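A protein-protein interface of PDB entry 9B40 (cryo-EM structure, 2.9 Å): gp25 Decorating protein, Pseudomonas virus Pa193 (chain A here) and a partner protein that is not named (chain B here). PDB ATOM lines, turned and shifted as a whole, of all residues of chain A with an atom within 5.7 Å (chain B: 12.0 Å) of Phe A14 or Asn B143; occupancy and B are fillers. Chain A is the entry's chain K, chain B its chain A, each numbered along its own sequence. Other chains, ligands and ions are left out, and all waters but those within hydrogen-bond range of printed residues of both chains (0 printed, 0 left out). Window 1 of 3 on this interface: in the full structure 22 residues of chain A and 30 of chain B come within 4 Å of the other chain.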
ATOM      1  N   THR A  11     -10.101 -22.935  19.267  1.00  0.00           N
ATOM      2  CA  THR A  11      -8.772 -22.725  18.714  1.00  0.00           C
ATOM      3  C   THR A  11      -8.324 -23.979  17.964  1.00  0.00           C
ATOM      4  O   THR A  11      -8.704 -25.093  18.335  1.00  0.00           O
ATOM      5  CB  THR A  11      -7.778 -22.371  19.824  1.00  0.00           C
ATOM      6  OG1 THR A  11      -6.466 -22.218  19.270  1.00  0.00           O
ATOM      7  CG2 THR A  11      -7.754 -23.439  20.907  1.00  0.00           C
ATOM      8  N   PRO A  12      -7.577 -23.829  16.867  1.00  0.00           N
ATOM      9  CA  PRO A  12      -7.101 -25.021  16.144  1.00  0.00           C
ATOM     10  C   PRO A  12      -6.187 -25.918  16.964  1.00  0.00           C
ATOM     11  O   PRO A  12      -6.164 -27.132  16.732  1.00  0.00           O
ATOM     12  CB  PRO A  12      -6.375 -24.429  14.928  1.00  0.00           C
ATOM     13  CG  PRO A  12      -6.949 -23.069  14.761  1.00  0.00           C
ATOM     14  CD  PRO A  12      -7.309 -22.584  16.129  1.00  0.00           C
ATOM     15  N   GLY A  13      -5.432 -25.365  17.904  1.00  0.00           N
ATOM     16  CA  GLY A  13      -4.583 -26.192  18.742  1.00  0.00           C
ATOM     17  C   GLY A  13      -3.830 -25.346  19.743  1.00  0.00           C
ATOM     18  O   GLY A  13      -3.938 -24.116  19.764  1.00  0.00           O
ATOM     19  N   PHE A  14      -3.053 -26.035  20.582  1.00  0.00           N
ATOM     20  CA  PHE A  14      -2.205 -25.431  21.594  1.00  0.00           C
ATOM     21  C   PHE A  14      -0.739 -25.609  21.215  1.00  0.00           C
ATOM     22  O   PHE A  14      -0.389 -26.599  20.568  1.00  0.00           O
ATOM     23  CB  PHE A  14      -2.455 -26.062  22.970  1.00  0.00           C
ATOM     24  CG  PHE A  14      -3.886 -26.018  23.404  1.00  0.00           C
ATOM     25  CD1 PHE A  14      -4.426 -24.864  23.945  1.00  0.00           C
ATOM     26  CD2 PHE A  14      -4.689 -27.138  23.290  1.00  0.00           C
ATOM     27  CE1 PHE A  14      -5.743 -24.825  24.348  1.00  0.00           C
ATOM     28  CE2 PHE A  14      -6.003 -27.106  23.696  1.00  0.00           C
ATOM     29  CZ  PHE A  14      -6.532 -25.947  24.223  1.00  0.00           C
ATOM     30  N   PRO A  15       0.139 -24.671  21.586  1.00  0.00           N
ATOM     31  CA  PRO A  15       1.540 -24.759  21.146  1.00  0.00           C
ATOM     32  C   PRO A  15       2.240 -26.009  21.660  1.00  0.00           C
ATOM     33  O   PRO A  15       2.030 -26.445  22.793  1.00  0.00           O
ATOM     34  CB  PRO A  15       2.176 -23.483  21.709  1.00  0.00           C
ATOM     35  CG  PRO A  15       1.248 -22.976  22.732  1.00  0.00           C
ATOM     36  CD  PRO A  15      -0.116 -23.479  22.412  1.00  0.00           C
ATOM     37  N   GLY A  16       3.088 -26.580  20.803  1.00  0.00           N
ATOM     38  CA  GLY A  16       3.750 -27.833  21.081  1.00  0.00           C
ATOM     39  C   GLY A  16       3.010 -29.068  20.616  1.00  0.00           C
ATOM     40  O   GLY A  16       3.536 -30.178  20.763  1.00  0.00           O
ATOM     41  N   ASP A  17       1.812 -28.917  20.062  1.00  0.00           N
ATOM     42  CA  ASP A  17       0.973 -30.041  19.677  1.00  0.00           C
ATOM     43  C   ASP A  17       1.010 -30.277  18.171  1.00  0.00           C
ATOM     44  O   ASP A  17       1.462 -29.438  17.389  1.00  0.00           O
ATOM     45  CB  ASP A  17      -0.463 -29.804  20.145  1.00  0.00           C
ATOM     46  CG  ASP A  17      -0.818 -30.641  21.345  1.00  0.00           C
ATOM     47  OD1 ASP A  17       0.106 -31.112  22.028  1.00  0.00           O
ATOM     48  OD2 ASP A  17      -2.016 -30.811  21.628  1.00  0.00           O
ATOM     49  N   LEU A  18       0.505 -31.441  17.772  1.00  0.00           N
ATOM     50  CA  LEU A  18       0.440 -31.844  16.374  1.00  0.00           C
ATOM     51  C   LEU A  18      -0.978 -31.632  15.861  1.00  0.00           C
ATOM     52  O   LEU A  18      -1.934 -32.158  16.440  1.00  0.00           O
ATOM     53  CB  LEU A  18       0.839 -33.311  16.212  1.00  0.00           C
ATOM     54  CG  LEU A  18       2.160 -33.639  15.519  1.00  0.00           C
ATOM     55  CD1 LEU A  18       3.270 -32.887  16.163  1.00  0.00           C
ATOM     56  CD2 LEU A  18       2.447 -35.118  15.571  1.00  0.00           C
ATOM     57  N   LYS A  92       1.292 -33.480  26.785  1.00  0.00           N
ATOM     58  CA  LYS A  92       0.586 -34.525  27.516  1.00  0.00           C
ATOM     59  C   LYS A  92       1.515 -35.631  28.000  1.00  0.00           C
ATOM     60  O   LYS A  92       1.104 -36.451  28.828  1.00  0.00           O
ATOM     61  CB  LYS A  92      -0.517 -35.110  26.638  1.00  0.00           C
ATOM     62  CG  LYS A  92      -1.337 -34.060  25.914  1.00  0.00           C
ATOM     63  CD  LYS A  92      -2.730 -34.565  25.592  1.00  0.00           C
ATOM     64  CE  LYS A  92      -3.579 -33.482  24.950  1.00  0.00           C
ATOM     65  NZ  LYS A  92      -2.846 -32.195  24.815  1.00  0.00           N
ATOM     66  N   TYR A 108       3.832 -24.418  31.634  1.00  0.00           N
ATOM     67  CA  TYR A 108       4.297 -24.993  30.380  1.00  0.00           C
ATOM     68  C   TYR A 108       5.807 -25.187  30.380  1.00  0.00           C
ATOM     69  O   TYR A 108       6.409 -25.372  29.319  1.00  0.00           O
ATOM     70  CB  TYR A 108       3.871 -24.112  29.207  1.00  0.00           C
ATOM     71  CG  TYR A 108       3.092 -24.837  28.139  1.00  0.00           C
ATOM     72  CD1 TYR A 108       2.272 -25.908  28.458  1.00  0.00           C
ATOM     73  CD2 TYR A 108       3.153 -24.431  26.815  1.00  0.00           C
ATOM     74  CE1 TYR A 108       1.550 -26.568  27.488  1.00  0.00           C
ATOM     75  CE2 TYR A 108       2.434 -25.086  25.836  1.00  0.00           C
ATOM     76  CZ  TYR A 108       1.635 -26.153  26.179  1.00  0.00           C
ATOM     77  OH  TYR A 108       0.916 -26.808  25.210  1.00  0.00           O
ATOM     78  N   VAL A 126       2.016 -26.960  16.170  1.00  0.00           N
ATOM     79  CA  VAL A 126       1.666 -25.646  16.692  1.00  0.00           C
ATOM     80  C   VAL A 126       2.855 -25.127  17.484  1.00  0.00           C
ATOM     81  O   VAL A 126       3.298 -25.758  18.447  1.00  0.00           O
ATOM     82  CB  VAL A 126       0.406 -25.697  17.566  1.00  0.00           C
ATOM     83  CG1 VAL A 126      -0.075 -24.293  17.865  1.00  0.00           C
ATOM     84  CG2 VAL A 126      -0.671 -26.471  16.886  1.00  0.00           C
ATOM     85  N   THR A 205       0.125 -18.324  18.114  1.00  0.00           N
ATOM     86  CA  THR A 205       0.595 -19.661  17.788  1.00  0.00           C
ATOM     87  C   THR A 205       0.237 -20.011  16.350  1.00  0.00           C
ATOM     88  O   THR A 205      -0.786 -19.574  15.816  1.00  0.00           O
ATOM     89  CB  THR A 205      -0.007 -20.687  18.746  1.00  0.00           C
ATOM     90  OG1 THR A 205      -1.388 -20.880  18.431  1.00  0.00           O
ATOM     91  CG2 THR A 205       0.106 -20.202  20.179  1.00  0.00           C
ATOM     92  N   GLN B 119     -11.803 -28.353  41.044  1.00  0.00           N
ATOM     93  CA  GLN B 119     -12.660 -28.421  39.869  1.00  0.00           C
ATOM     94  C   GLN B 119     -11.804 -28.242  38.625  1.00  0.00           C
ATOM     95  O   GLN B 119     -10.968 -27.335  38.569  1.00  0.00           O
ATOM     96  CB  GLN B 119     -13.751 -27.349  39.922  1.00  0.00           C
ATOM     97  CG  GLN B 119     -14.587 -27.223  38.656  1.00  0.00           C
ATOM     98  CD  GLN B 119     -15.369 -28.479  38.337  1.00  0.00           C
ATOM     99  OE1 GLN B 119     -14.934 -29.308  37.540  1.00  0.00           O
ATOM    100  NE2 GLN B 119     -16.535 -28.620  38.951  1.00  0.00           N
ATOM    101  N   GLY B 120     -12.014 -29.097  37.630  1.00  0.00           N
ATOM    102  CA  GLY B 120     -11.217 -29.082  36.414  1.00  0.00           C
ATOM    103  C   GLY B 120     -11.963 -28.453  35.251  1.00  0.00           C
ATOM    104  O   GLY B 120     -13.147 -28.712  35.042  1.00  0.00           O
ATOM    105  N   ILE B 121     -11.246 -27.626  34.494  1.00  0.00           N
ATOM    106  CA  ILE B 121     -11.755 -26.992  33.283  1.00  0.00           C
ATOM    107  C   ILE B 121     -10.886 -27.459  32.122  1.00  0.00           C
ATOM    108  O   ILE B 121      -9.675 -27.210  32.105  1.00  0.00           O
ATOM    109  CB  ILE B 121     -11.764 -25.456  33.405  1.00  0.00           C
ATOM    110  CG1 ILE B 121     -11.930 -24.775  32.042  1.00  0.00           C
ATOM    111  CG2 ILE B 121     -10.541 -24.947  34.157  1.00  0.00           C
ATOM    112  CD1 ILE B 121     -13.255 -25.022  31.373  1.00  0.00           C
ATOM    113  N   VAL B 122     -11.496 -28.148  31.165  1.00  0.00           N
ATOM    114  CA  VAL B 122     -10.781 -28.719  30.029  1.00  0.00           C
ATOM    115  C   VAL B 122     -11.189 -27.942  28.787  1.00  0.00           C
ATOM    116  O   VAL B 122     -12.357 -27.966  28.381  1.00  0.00           O
ATOM    117  CB  VAL B 122     -11.067 -30.217  29.866  1.00  0.00           C
ATOM    118  CG1 VAL B 122     -10.590 -30.704  28.508  1.00  0.00           C
ATOM    119  CG2 VAL B 122     -10.400 -31.005  30.975  1.00  0.00           C
ATOM    120  N   GLU B 123     -10.231 -27.247  28.185  1.00  0.00           N
ATOM    121  CA  GLU B 123     -10.463 -26.573  26.917  1.00  0.00           C
ATOM    122  C   GLU B 123     -10.044 -27.485  25.776  1.00  0.00           C
ATOM    123  O   GLU B 123      -8.859 -27.834  25.683  1.00  0.00           O
ATOM    124  CB  GLU B 123      -9.686 -25.274  26.842  1.00  0.00           C
ATOM    125  CG  GLU B 123      -9.697 -24.648  25.462  1.00  0.00           C
ATOM    126  CD  GLU B 123      -9.367 -23.174  25.486  1.00  0.00           C
ATOM    127  OE1 GLU B 123      -8.547 -22.763  26.331  1.00  0.00           O
ATOM    128  OE2 GLU B 123      -9.926 -22.426  24.659  1.00  0.00           O
ATOM    129  N   PRO B 124     -10.957 -27.897  24.906  1.00  0.00           N
ATOM    130  CA  PRO B 124     -10.577 -28.691  23.740  1.00  0.00           C
ATOM    131  C   PRO B 124     -10.194 -27.789  22.571  1.00  0.00           C
ATOM    132  O   PRO B 124     -10.367 -26.571  22.606  1.00  0.00           O
ATOM    133  CB  PRO B 124     -11.852 -29.483  23.438  1.00  0.00           C
ATOM    134  CG  PRO B 124     -12.953 -28.590  23.895  1.00  0.00           C
ATOM    135  CD  PRO B 124     -12.416 -27.731  25.012  1.00  0.00           C
ATOM    136  N   ALA B 125      -9.668 -28.419  21.525  1.00  0.00           N
ATOM    137  CA  ALA B 125      -9.165 -27.670  20.385  1.00  0.00           C
ATOM    138  C   ALA B 125      -9.209 -28.545  19.147  1.00  0.00           C
ATOM    139  O   ALA B 125      -8.994 -29.757  19.218  1.00  0.00           O
ATOM    140  CB  ALA B 125      -7.736 -27.177  20.628  1.00  0.00           C
ATOM    141  N   GLY B 126      -9.475 -27.910  18.010  1.00  0.00           N
ATOM    142  CA  GLY B 126      -9.507 -28.607  16.742  1.00  0.00           C
ATOM    143  C   GLY B 126     -10.384 -27.925  15.717  1.00  0.00           C
ATOM    144  O   GLY B 126     -11.492 -27.482  16.029  1.00  0.00           O
ATOM    145  N   THR B 127      -9.892 -27.831  14.488  1.00  0.00           N
ATOM    146  CA  THR B 127     -10.646 -27.279  13.375  1.00  0.00           C
ATOM    147  C   THR B 127     -10.663 -28.295  12.248  1.00  0.00           C
ATOM    148  O   THR B 127      -9.646 -28.933  11.963  1.00  0.00           O
ATOM    149  CB  THR B 127     -10.045 -25.962  12.873  1.00  0.00           C
ATOM    150  OG1 THR B 127      -8.628 -26.110  12.723  1.00  0.00           O
ATOM    151  CG2 THR B 127     -10.331 -24.836  13.850  1.00  0.00           C
ATOM    152  N   PRO B 138      -6.089 -33.857   9.982  1.00  0.00           N
ATOM    153  CA  PRO B 138      -6.072 -32.914  11.102  1.00  0.00           C
ATOM    154  C   PRO B 138      -6.365 -33.633  12.408  1.00  0.00           C
ATOM    155  O   PRO B 138      -7.086 -34.630  12.438  1.00  0.00           O
ATOM    156  CB  PRO B 138      -7.186 -31.925  10.748  1.00  0.00           C
ATOM    157  CG  PRO B 138      -8.120 -32.726   9.920  1.00  0.00           C
ATOM    158  CD  PRO B 138      -7.259 -33.655   9.113  1.00  0.00           C
ATOM    159  N   LEU B 139      -5.794 -33.123  13.498  1.00  0.00           N
ATOM    160  CA  LEU B 139      -5.922 -33.778  14.793  1.00  0.00           C
ATOM    161  C   LEU B 139      -6.430 -32.794  15.835  1.00  0.00           C
ATOM    162  O   LEU B 139      -5.997 -31.639  15.878  1.00  0.00           O
ATOM    163  CB  LEU B 139      -4.590 -34.382  15.258  1.00  0.00           C
ATOM    164  CG  LEU B 139      -3.891 -35.365  14.312  1.00  0.00           C
ATOM    165  CD1 LEU B 139      -2.455 -35.599  14.748  1.00  0.00           C
ATOM    166  CD2 LEU B 139      -4.645 -36.670  14.184  1.00  0.00           C
ATOM    167  N   THR B 140      -7.351 -33.261  16.673  1.00  0.00           N
ATOM    168  CA  THR B 140      -7.856 -32.495  17.800  1.00  0.00           C
ATOM    169  C   THR B 140      -6.977 -32.715  19.026  1.00  0.00           C
ATOM    170  O   THR B 140      -6.123 -33.604  19.058  1.00  0.00           O
ATOM    171  CB  THR B 140      -9.299 -32.883  18.112  1.00  0.00           C
ATOM    172  OG1 THR B 140      -9.344 -34.244  18.555  1.00  0.00           O
ATOM    173  CG2 THR B 140     -10.161 -32.738  16.887  1.00  0.00           C
ATOM    174  N   SER B 141      -7.197 -31.895  20.049  1.00  0.00           N
ATOM    175  CA  SER B 141      -6.443 -32.003  21.293  1.00  0.00           C
ATOM    176  C   SER B 141      -7.218 -31.302  22.402  1.00  0.00           C
ATOM    177  O   SER B 141      -8.371 -30.898  22.216  1.00  0.00           O
ATOM    178  CB  SER B 141      -5.040 -31.415  21.136  1.00  0.00           C
ATOM    179  OG  SER B 141      -5.077 -30.000  21.162  1.00  0.00           O
ATOM    180  N   TRP B 142      -6.571 -31.137  23.553  1.00  0.00           N
ATOM    181  CA  TRP B 142      -7.188 -30.506  24.711  1.00  0.00           C
ATOM    182  C   TRP B 142      -6.101 -30.086  25.688  1.00  0.00           C
ATOM    183  O   TRP B 142      -4.952 -30.523  25.592  1.00  0.00           O
ATOM    184  CB  TRP B 142      -8.185 -31.449  25.391  1.00  0.00           C
ATOM    185  CG  TRP B 142      -7.583 -32.769  25.748  1.00  0.00           C
ATOM    186  CD1 TRP B 142      -7.569 -33.893  24.979  1.00  0.00           C
ATOM    187  CD2 TRP B 142      -6.894 -33.103  26.956  1.00  0.00           C
ATOM    188  NE1 TRP B 142      -6.919 -34.908  25.634  1.00  0.00           N
ATOM    189  CE2 TRP B 142      -6.493 -34.447  26.851  1.00  0.00           C
ATOM    190  CE3 TRP B 142      -6.579 -32.396  28.120  1.00  0.00           C
ATOM    191  CZ2 TRP B 142      -5.796 -35.098  27.863  1.00  0.00           C
ATOM    192  CZ3 TRP B 142      -5.888 -33.042  29.120  1.00  0.00           C
ATOM    193  CH2 TRP B 142      -5.502 -34.378  28.986  1.00  0.00           C
ATOM    194  N   ASN B 143      -6.480 -29.222  26.627  1.00  0.00           N
ATOM    195  CA  ASN B 143      -5.638 -28.899  27.771  1.00  0.00           C
ATOM    196  C   ASN B 143      -6.526 -28.701  28.991  1.00  0.00           C
ATOM    197  O   ASN B 143      -7.732 -28.485  28.869  1.00  0.00           O
ATOM    198  CB  ASN B 143      -4.743 -27.674  27.503  1.00  0.00           C
ATOM    199  CG  ASN B 143      -5.428 -26.351  27.793  1.00  0.00           C
ATOM    200  OD1 ASN B 143      -4.821 -25.407  28.297  1.00  0.00           O
ATOM    201  ND2 ASN B 143      -6.711 -26.279  27.467  1.00  0.00           N
ATOM    202  N   ALA B 144      -5.930 -28.796  30.177  1.00  0.00           N
ATOM    203  CA  ALA B 144      -6.706 -28.768  31.410  1.00  0.00           C
ATOM    204  C   ALA B 144      -6.096 -27.815  32.425  1.00  0.00           C
ATOM    205  O   ALA B 144      -4.874 -27.756  32.586  1.00  0.00           O
ATOM    206  CB  ALA B 144      -6.819 -30.166  32.020  1.00  0.00           C
ATOM    207  N   ASN B 145      -6.968 -27.081  33.114  1.00  0.00           N
ATOM    208  CA  ASN B 145      -6.613 -26.233  34.240  1.00  0.00           C
ATOM    209  C   ASN B 145      -7.452 -26.657  35.436  1.00  0.00           C
ATOM    210  O   ASN B 145      -8.489 -27.304  35.290  1.00  0.00           O
ATOM    211  CB  ASN B 145      -6.851 -24.748  33.940  1.00  0.00           C
ATOM    212  CG  ASN B 145      -5.853 -24.180  32.956  1.00  0.00           C
ATOM    213  OD1 ASN B 145      -5.150 -24.916  32.269  1.00  0.00           O
ATOM    214  ND2 ASN B 145      -5.790 -22.859  32.881  1.00  0.00           N
ATOM    215  N   PHE B 146      -6.996 -26.295  36.632  1.00  0.00           N
ATOM    216  CA  PHE B 146      -7.661 -26.735  37.847  1.00  0.00           C
ATOM    217  C   PHE B 146      -7.786 -25.575  38.821  1.00  0.00           C
ATOM    218  O   PHE B 146      -6.899 -24.724  38.916  1.00  0.00           O
ATOM    219  CB  PHE B 146      -6.905 -27.899  38.498  1.00  0.00           C
ATOM    220  CG  PHE B 146      -6.569 -29.006  37.542  1.00  0.00           C
ATOM    221  CD1 PHE B 146      -7.538 -29.901  37.129  1.00  0.00           C
ATOM    222  CD2 PHE B 146      -5.287 -29.137  37.040  1.00  0.00           C
ATOM    223  CE1 PHE B 146      -7.232 -30.917  36.247  1.00  0.00           C
ATOM    224  CE2 PHE B 146      -4.977 -30.147  36.154  1.00  0.00           C
ATOM    225  CZ  PHE B 146      -5.951 -31.039  35.758  1.00  0.00           C
ATOM    226  N   GLU B 147      -8.893 -25.564  39.559  1.00  0.00           N
ATOM    227  CA  GLU B 147      -9.177 -24.539  40.553  1.00  0.00           C
ATOM    228  C   GLU B 147      -9.424 -25.200  41.897  1.00  0.00           C
ATOM    229  O   GLU B 147     -10.231 -26.128  41.996  1.00  0.00           O
ATOM    230  CB  GLU B 147     -10.389 -23.693  40.152  1.00  0.00           C
ATOM    231  CG  GLU B 147     -10.747 -22.565  41.120  1.00  0.00           C
ATOM    232  CD  GLU B 147      -9.724 -21.440  41.171  1.00  0.00           C
ATOM    233  OE1 GLU B 147      -8.608 -21.648  41.692  1.00  0.00           O
ATOM    234  OE2 GLU B 147     -10.043 -20.332  40.690  1.00  0.00           O
ATOM    235  N   ASP B 328     -21.406 -28.314  24.445  1.00  0.00           N
ATOM    236  CA  ASP B 328     -19.987 -28.281  24.766  1.00  0.00           C
ATOM    237  C   ASP B 328     -19.409 -29.624  25.186  1.00  0.00           C
ATOM    238  O   ASP B 328     -18.183 -29.771  25.186  1.00  0.00           O
ATOM    239  CB  ASP B 328     -19.719 -27.259  25.881  1.00  0.00           C
ATOM    240  CG  ASP B 328     -20.634 -27.441  27.072  1.00  0.00           C
ATOM    241  OD1 ASP B 328     -21.735 -28.001  26.898  1.00  0.00           O
ATOM    242  OD2 ASP B 328     -20.255 -27.016  28.185  1.00  0.00           O
ATOM    243  N   GLY B 329     -20.243 -30.597  25.537  1.00  0.00           N
ATOM    244  CA  GLY B 329     -19.742 -31.872  26.004  1.00  0.00           C
ATOM    245  C   GLY B 329     -19.299 -31.895  27.447  1.00  0.00           C
ATOM    246  O   GLY B 329     -18.602 -32.834  27.848  1.00  0.00           O
ATOM    247  N   SER B 330     -19.663 -30.884  28.235  1.00  0.00           N
ATOM    248  CA  SER B 330     -19.294 -30.854  29.644  1.00  0.00           C
ATOM    249  C   SER B 330     -19.972 -31.986  30.404  1.00  0.00           C
ATOM    250  O   SER B 330     -21.161 -32.256  30.222  1.00  0.00           O
ATOM    251  CB  SER B 330     -19.681 -29.513  30.265  1.00  0.00           C
ATOM    252  OG  SER B 330     -18.765 -28.495  29.911  1.00  0.00           O
ATOM    253  N   THR B 331     -19.206 -32.647  31.268  1.00  0.00           N
ATOM    254  CA  THR B 331     -19.722 -33.711  32.118  1.00  0.00           C
ATOM    255  C   THR B 331     -19.730 -33.316  33.590  1.00  0.00           C
ATOM    256  O   THR B 331     -19.864 -34.181  34.460  1.00  0.00           O
ATOM    257  CB  THR B 331     -18.914 -34.990  31.916  1.00  0.00           C
ATOM    258  OG1 THR B 331     -19.203 -35.913  32.974  1.00  0.00           O
ATOM    259  CG2 THR B 331     -17.427 -34.683  31.896  1.00  0.00           C
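Thr A11 touches Ala B125.
Gly B126 touches Pro A12 (N to O, 3.6 Å).
OG1 of Thr B127 touches CB of Pro A12, at 3.6 Å.
Ala B125 touches Gly A13 (CB to CA, 3.8 Å).
CZ of Phe A14 touches O of Glu B123, at 3.3 Å.
CE2 of Phe A14 touches CB of Ala B125, at 3.5 Å.
Phe A14 touches Ser B141.
Trp B142 touches Phe A14.
Phe A14 touches Asn B143.
Leu A18 touches Leu B139 (O to CB, 3.7 Å).
Thr A11 touches just these residues of chain B: Ala B125 and Gly B126.
Pro A12 touches just these residues of chain B: Gly B126 and Thr B127.
Of the printed residues of chain B, Gly A13 touches Ala B125.
No residue of chain B comes within 4 Å of Gly A16.
No residue of chain B comes within 4 Å of Val A126.
Of the printed residues of chain A, Thr B127 touches Pro A12 (3.6 Å).
Thr B140 touches none of the printed residues of chain A.
Of the printed residues of chain A, Ser B141 touches Phe A14 and Asp A17.
Asn B143 touches one residue of chain A.
The nearest residue of chain B that does not touch Phe A14 is Pro B124 (4.2 Å).
The nearest printed residue of chain A that does not touch Thr B127 is Thr A11 (4.7 Å).
The backbone NH (N) of Gly B126 is in hydrogen-bond range of the backbone carbonyl oxygen (O) of Thr A11 (2.9 Å).
OG of Ser B141 lies close to OD2 of Asp A17 (3.2 Å).
The side-chain amino group (NZ) of Lys A92 is in hydrogen-bond range of the backbone carbonyl oxygen (O) of Trp B142.
N of Glu B123 sits at hydrogen-bond distance from O of Asn B143 (2.9 Å).
O of Ser B141 lies within hydrogen-bond range of N of Ala B125, at 2.9 Å.
OG1 of Thr A11 is in hydrogen-bond range of O of Gly A13 (3.2 Å).
The side-chain carboxylate of Asp A17 is in salt-bridge range of the side-chain amino group of Lys A92 (3.6 Å).
O of Asp A17 is in hydrogen-bond range of N of Val A126, 2.8 Å away.
Of the 12 printed residues of chain A, 7 touch a printed residue of chain B.
Hydrophobic or aromatic side chains of chain A within 4 Å of the printed part of chain B: Pro A12 and Phe A14.
Along chain A the printed residues that touch a printed residue of chain B span positions 11 to 92.
Of the 23 printed residues of chain B, 8 touch a printed residue of chain A.
Printed residues of chain B that touch a printed residue of chain A: Glu B123, Ala B125, Gly B126, Thr B127, Leu B139, Ser B141, Trp B142 and Asn B143.
Hydrophobic or aromatic side chains of chain B within 4 Å of the printed part of chain A: Ala B125, Leu B139 and Trp B142.
Along chain B the printed residues that touch a printed residue of chain A span positions 123 to 143.
Among the printed residues, 13 pairs touch across the chains.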
